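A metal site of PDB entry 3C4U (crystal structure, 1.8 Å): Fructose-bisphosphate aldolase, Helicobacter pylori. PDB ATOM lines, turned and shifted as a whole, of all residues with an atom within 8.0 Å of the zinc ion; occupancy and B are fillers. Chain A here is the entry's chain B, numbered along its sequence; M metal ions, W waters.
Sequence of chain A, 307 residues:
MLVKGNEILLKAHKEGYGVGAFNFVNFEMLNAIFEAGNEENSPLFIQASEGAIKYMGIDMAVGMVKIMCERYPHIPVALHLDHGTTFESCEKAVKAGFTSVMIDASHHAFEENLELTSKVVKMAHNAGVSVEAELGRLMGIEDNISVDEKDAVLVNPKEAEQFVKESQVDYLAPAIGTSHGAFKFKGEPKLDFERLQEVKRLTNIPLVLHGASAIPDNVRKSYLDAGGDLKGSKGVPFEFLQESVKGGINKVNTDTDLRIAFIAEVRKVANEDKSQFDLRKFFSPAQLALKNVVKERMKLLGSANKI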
ATOM      1  N   ASP A  82      29.362  29.527  -3.373  1.00  0.00           N
ATOM      2  CA  ASP A  82      27.998  29.056  -3.529  1.00  0.00           C
ATOM      3  C   ASP A  82      27.938  27.547  -3.726  1.00  0.00           C
ATOM      4  O   ASP A  82      28.449  27.025  -4.716  1.00  0.00           O
ATOM      5  CB  ASP A  82      27.334  29.760  -4.711  1.00  0.00           C
ATOM      6  CG  ASP A  82      25.862  29.394  -4.855  1.00  0.00           C
ATOM      7  OD1 ASP A  82      25.301  28.798  -3.916  1.00  0.00           O
ATOM      8  OD2 ASP A  82      25.275  29.706  -5.913  1.00  0.00           O
ATOM      9  N   HIS A  83      27.320  26.863  -2.772  1.00  0.00           N
ATOM     10  CA  HIS A  83      27.118  25.414  -2.845  1.00  0.00           C
ATOM     11  C   HIS A  83      28.408  24.625  -3.050  1.00  0.00           C
ATOM     12  O   HIS A  83      28.535  23.875  -4.018  1.00  0.00           O
ATOM     13  CB  HIS A  83      26.120  25.057  -3.946  1.00  0.00           C
ATOM     14  CG  HIS A  83      24.698  25.280  -3.560  1.00  0.00           C
ATOM     15  ND1 HIS A  83      24.075  26.505  -3.664  1.00  0.00           N
ATOM     16  CD2 HIS A  83      23.759  24.426  -3.069  1.00  0.00           C
ATOM     17  CE1 HIS A  83      22.828  26.398  -3.252  1.00  0.00           C
ATOM     18  NE2 HIS A  83      22.604  25.150  -2.887  1.00  0.00           N
ATOM     19  N   MET A 102      29.987  28.021   1.617  1.00  0.00           N
ATOM     20  CA  MET A 102      28.877  27.123   1.901  1.00  0.00           C
ATOM     21  C   MET A 102      29.267  25.686   1.609  1.00  0.00           C
ATOM     22  O   MET A 102      29.810  25.391   0.545  1.00  0.00           O
ATOM     23  CB  MET A 102      27.638  27.480   1.081  1.00  0.00           C
ATOM     24  CG  MET A 102      26.407  26.695   1.496  1.00  0.00           C
ATOM     25  SD  MET A 102      25.445  26.034   0.125  1.00  0.00           S
ATOM     26  CE  MET A 102      24.219  25.088   1.026  1.00  0.00           C
ATOM     27  N   ASP A 104      27.478  22.163   1.103  1.00  0.00           N
ATOM     28  CA  ASP A 104      26.180  21.541   0.903  1.00  0.00           C
ATOM     29  C   ASP A 104      26.256  20.032   1.027  1.00  0.00           C
ATOM     30  O   ASP A 104      26.702  19.332   0.117  1.00  0.00           O
ATOM     31  CB  ASP A 104      25.599  21.919  -0.456  1.00  0.00           C
ATOM     32  CG  ASP A 104      24.205  21.358  -0.675  1.00  0.00           C
ATOM     33  OD1 ASP A 104      23.586  20.915   0.315  1.00  0.00           O
ATOM     34  OD2 ASP A 104      23.742  21.366  -1.825  1.00  0.00           O
ATOM     35  N   SER A 106      23.340  18.516   2.315  1.00  0.00           N
ATOM     36  CA  SER A 106      21.939  18.346   2.673  1.00  0.00           C
ATOM     37  C   SER A 106      21.329  17.097   2.034  1.00  0.00           C
ATOM     38  O   SER A 106      20.219  16.680   2.402  1.00  0.00           O
ATOM     39  CB  SER A 106      21.129  19.583   2.287  1.00  0.00           C
ATOM     40  OG  SER A 106      21.176  19.812   0.885  1.00  0.00           O
ATOM     41  N   GLU A 132      28.249  28.590   5.696  1.00  0.00           N
ATOM     42  CA  GLU A 132      26.828  28.310   5.531  1.00  0.00           C
ATOM     43  C   GLU A 132      26.612  26.824   5.302  1.00  0.00           C
ATOM     44  O   GLU A 132      27.449  26.151   4.695  1.00  0.00           O
ATOM     45  CB  GLU A 132      26.260  29.106   4.352  1.00  0.00           C
ATOM     46  CG  GLU A 132      24.804  28.785   4.053  1.00  0.00           C
ATOM     47  CD  GLU A 132      24.304  29.472   2.802  1.00  0.00           C
ATOM     48  OE1 GLU A 132      24.817  30.558   2.469  1.00  0.00           O
ATOM     49  OE2 GLU A 132      23.399  28.916   2.145  1.00  0.00           O
ATOM     50  N   ALA A 133      25.484  26.314   5.779  1.00  0.00           N
ATOM     51  CA  ALA A 133      25.114  24.917   5.573  1.00  0.00           C
ATOM     52  C   ALA A 133      23.654  24.814   5.168  1.00  0.00           C
ATOM     53  O   ALA A 133      22.926  25.804   5.162  1.00  0.00           O
ATOM     54  CB  ALA A 133      25.390  24.109   6.820  1.00  0.00           C
ATOM     55  N   GLU A 134      23.224  23.601   4.836  1.00  0.00           N
ATOM     56  CA  GLU A 134      21.850  23.372   4.419  1.00  0.00           C
ATOM     57  C   GLU A 134      21.270  22.126   5.088  1.00  0.00           C
ATOM     58  O   GLU A 134      21.980  21.146   5.294  1.00  0.00           O
ATOM     59  CB  GLU A 134      21.772  23.237   2.899  1.00  0.00           C
ATOM     60  CG  GLU A 134      20.363  23.253   2.341  1.00  0.00           C
ATOM     61  CD  GLU A 134      20.353  23.508   0.857  1.00  0.00           C
ATOM     62  OE1 GLU A 134      21.443  23.723   0.298  1.00  0.00           O
ATOM     63  OE2 GLU A 134      19.260  23.486   0.248  1.00  0.00           O
ATOM     64  N   LEU A 135      20.002  22.161   5.434  1.00  0.00           N
ATOM     65  CA  LEU A 135      19.367  21.059   6.151  1.00  0.00           C
ATOM     66  C   LEU A 135      17.889  20.949   5.783  1.00  0.00           C
ATOM     67  O   LEU A 135      17.177  21.952   5.755  1.00  0.00           O
ATOM     68  CB  LEU A 135      19.518  21.254   7.664  1.00  0.00           C
ATOM     69  CG  LEU A 135      18.957  20.148   8.543  1.00  0.00           C
ATOM     70  CD1 LEU A 135      19.672  18.837   8.249  1.00  0.00           C
ATOM     71  CD2 LEU A 135      19.084  20.511  10.017  1.00  0.00           C
ATOM     72  N   ALA A 173      20.656  27.223   5.718  1.00  0.00           N
ATOM     73  CA  ALA A 173      19.627  27.235   4.678  1.00  0.00           C
ATOM     74  C   ALA A 173      18.647  26.091   4.921  1.00  0.00           C
ATOM     75  O   ALA A 173      18.906  24.949   4.518  1.00  0.00           O
ATOM     76  CB  ALA A 173      20.267  27.122   3.298  1.00  0.00           C
ATOM     77  N   THR A 178      10.562  25.750  -0.752  1.00  0.00           N
ATOM     78  CA  THR A 178      11.064  25.864  -2.122  1.00  0.00           C
ATOM     79  C   THR A 178      11.436  24.497  -2.689  1.00  0.00           C
ATOM     80  O   THR A 178      11.989  23.648  -1.981  1.00  0.00           O
ATOM     81  CB  THR A 178      12.277  26.799  -2.211  1.00  0.00           C
ATOM     82  OG1 THR A 178      13.350  26.296  -1.408  1.00  0.00           O
ATOM     83  CG2 THR A 178      11.912  28.204  -1.740  1.00  0.00           C
ATOM     84  N   HIS A 180      13.929  22.682  -4.397  1.00  0.00           N
ATOM     85  CA  HIS A 180      15.335  22.946  -4.667  1.00  0.00           C
ATOM     86  C   HIS A 180      16.274  21.879  -4.110  1.00  0.00           C
ATOM     87  O   HIS A 180      16.008  21.278  -3.068  1.00  0.00           O
ATOM     88  CB  HIS A 180      15.713  24.318  -4.111  1.00  0.00           C
ATOM     89  CG  HIS A 180      17.180  24.485  -3.856  1.00  0.00           C
ATOM     90  ND1 HIS A 180      18.038  25.010  -4.799  1.00  0.00           N
ATOM     91  CD2 HIS A 180      17.934  24.191  -2.775  1.00  0.00           C
ATOM     92  CE1 HIS A 180      19.259  25.031  -4.302  1.00  0.00           C
ATOM     93  NE2 HIS A 180      19.227  24.534  -3.080  1.00  0.00           N
ATOM     94  N   GLY A 181      17.375  21.647  -4.821  1.00  0.00           N
ATOM     95  CA  GLY A 181      18.413  20.735  -4.374  1.00  0.00           C
ATOM     96  C   GLY A 181      17.917  19.348  -4.032  1.00  0.00           C
ATOM     97  O   GLY A 181      17.340  18.655  -4.875  1.00  0.00           O
ATOM     98  N   ALA A 182      18.161  18.936  -2.790  1.00  0.00           N
ATOM     99  CA  ALA A 182      17.768  17.606  -2.336  1.00  0.00           C
ATOM    100  C   ALA A 182      16.315  17.599  -1.862  1.00  0.00           C
ATOM    101  O   ALA A 182      15.828  16.594  -1.338  1.00  0.00           O
ATOM    102  CB  ALA A 182      18.687  17.145  -1.221  1.00  0.00           C
ATOM    103  N   PHE A 183      15.622  18.720  -2.054  1.00  0.00           N
ATOM    104  CA  PHE A 183      14.252  18.847  -1.590  1.00  0.00           C
ATOM    105  C   PHE A 183      13.307  19.233  -2.730  1.00  0.00           C
ATOM    106  O   PHE A 183      12.374  20.005  -2.535  1.00  0.00           O
ATOM    107  CB  PHE A 183      14.167  19.892  -0.483  1.00  0.00           C
ATOM    108  CG  PHE A 183      15.361  19.901   0.429  1.00  0.00           C
ATOM    109  CD1 PHE A 183      16.207  20.997   0.486  1.00  0.00           C
ATOM    110  CD2 PHE A 183      15.658  18.796   1.209  1.00  0.00           C
ATOM    111  CE1 PHE A 183      17.298  20.998   1.317  1.00  0.00           C
ATOM    112  CE2 PHE A 183      16.760  18.790   2.044  1.00  0.00           C
ATOM    113  CZ  PHE A 183      17.578  19.895   2.099  1.00  0.00           C
ATOM    114  N   VAL A 208      19.108  31.341   5.454  1.00  0.00           N
ATOM    115  CA  VAL A 208      19.315  31.517   4.027  1.00  0.00           C
ATOM    116  C   VAL A 208      18.223  30.841   3.202  1.00  0.00           C
ATOM    117  O   VAL A 208      17.768  29.751   3.533  1.00  0.00           O
ATOM    118  CB  VAL A 208      20.686  30.950   3.589  1.00  0.00           C
ATOM    119  CG1 VAL A 208      20.961  31.303   2.140  1.00  0.00           C
ATOM    120  CG2 VAL A 208      21.792  31.478   4.488  1.00  0.00           C
ATOM    121  N   LEU A 209      17.797  31.510   2.133  1.00  0.00           N
ATOM    122  CA  LEU A 209      16.746  30.987   1.278  1.00  0.00           C
ATOM    123  C   LEU A 209      17.291  30.561  -0.085  1.00  0.00           C
ATOM    124  O   LEU A 209      17.883  31.369  -0.803  1.00  0.00           O
ATOM    125  CB  LEU A 209      15.640  32.016   1.100  1.00  0.00           C
ATOM    126  CG  LEU A 209      14.419  31.583   0.284  1.00  0.00           C
ATOM    127  CD1 LEU A 209      13.740  30.386   0.926  1.00  0.00           C
ATOM    128  CD2 LEU A 209      13.433  32.740   0.148  1.00  0.00           C
ATOM    129  N   HIS A 210      17.069  29.294  -0.434  1.00  0.00           N
ATOM    130  CA  HIS A 210      17.536  28.750  -1.704  1.00  0.00           C
ATOM    131  C   HIS A 210      16.360  28.420  -2.617  1.00  0.00           C
ATOM    132  O   HIS A 210      15.261  28.120  -2.144  1.00  0.00           O
ATOM    133  CB  HIS A 210      18.366  27.489  -1.456  1.00  0.00           C
ATOM    134  CG  HIS A 210      19.688  27.751  -0.808  1.00  0.00           C
ATOM    135  ND1 HIS A 210      20.750  26.877  -0.887  1.00  0.00           N
ATOM    136  CD2 HIS A 210      20.133  28.805  -0.078  1.00  0.00           C
ATOM    137  CE1 HIS A 210      21.776  27.365  -0.222  1.00  0.00           C
ATOM    138  NE2 HIS A 210      21.425  28.543   0.273  1.00  0.00           N
ATOM    139  N   GLY A 211      16.603  28.459  -3.920  1.00  0.00           N
ATOM    140  CA  GLY A 211      15.611  28.074  -4.897  1.00  0.00           C
ATOM    141  C   GLY A 211      14.395  28.972  -4.945  1.00  0.00           C
ATOM    142  O   GLY A 211      13.286  28.528  -5.256  1.00  0.00           O
ATOM    143  N   ASN A 253      19.489  33.807  -2.055  1.00  0.00           N
ATOM    144  CA  ASN A 253      20.270  33.466  -3.248  1.00  0.00           C
ATOM    145  C   ASN A 253      19.604  33.942  -4.527  1.00  0.00           C
ATOM    146  O   ASN A 253      18.431  33.647  -4.781  1.00  0.00           O
ATOM    147  CB  ASN A 253      20.511  31.957  -3.307  1.00  0.00           C
ATOM    148  CG  ASN A 253      21.406  31.464  -2.201  1.00  0.00           C
ATOM    149  OD1 ASN A 253      21.542  32.108  -1.158  1.00  0.00           O
ATOM    150  ND2 ASN A 253      22.041  30.321  -2.411  1.00  0.00           N
HETATM  151 ZN    ZN M   1      20.819  24.596  -1.635  1.00  0.00          ZN
HETATM  152  O   HOH W   1      21.091  22.276  -2.369  1.00  0.00           O
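The side-chain sulfur (SD) of Met 102 lies close to the backbone NH (N) of His 83, at 3.5 Å.
A ring nitrogen (NE2) of His 210 lies within hydrogen-bond range of the side-chain carboxylate (OE2) of Glu 132, 2.7 Å away.
The side-chain carboxylate (OD1) of Asp 82 sits at hydrogen-bond distance from a ring nitrogen (ND1) of His 83, at 2.6 Å.
OG1 of Thr 178 lies within hydrogen-bond range of O of His 210, at 2.7 Å.
The side-chain amide nitrogen (ND2) of Asn 253 sits at hydrogen-bond distance from a ring nitrogen (NE2) of His 210.
A ring nitrogen (NE2) of His 180 binds the zinc ion, at 2.2 Å.
The side-chain carboxylate (OE1) of Glu 134 binds the zinc ion (2.2 Å).
The zinc ion is bound by a ring nitrogen (NE2) of His 83.
The zinc ion is bound by ND1 of His 210, 2.4 Å away.
The zinc ion is bound by water W1 (2.4 Å).
The zinc ion has five donor atoms within binding distance.
Slightly farther from the zinc ion lies OE2 of Glu 134 (2.7 Å).
Water W1 lies within hydrogen-bond range of the side-chain carboxylate of Asp 104 (2.9 Å) and the side-chain carboxylate of Glu 134 (3.4 Å).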
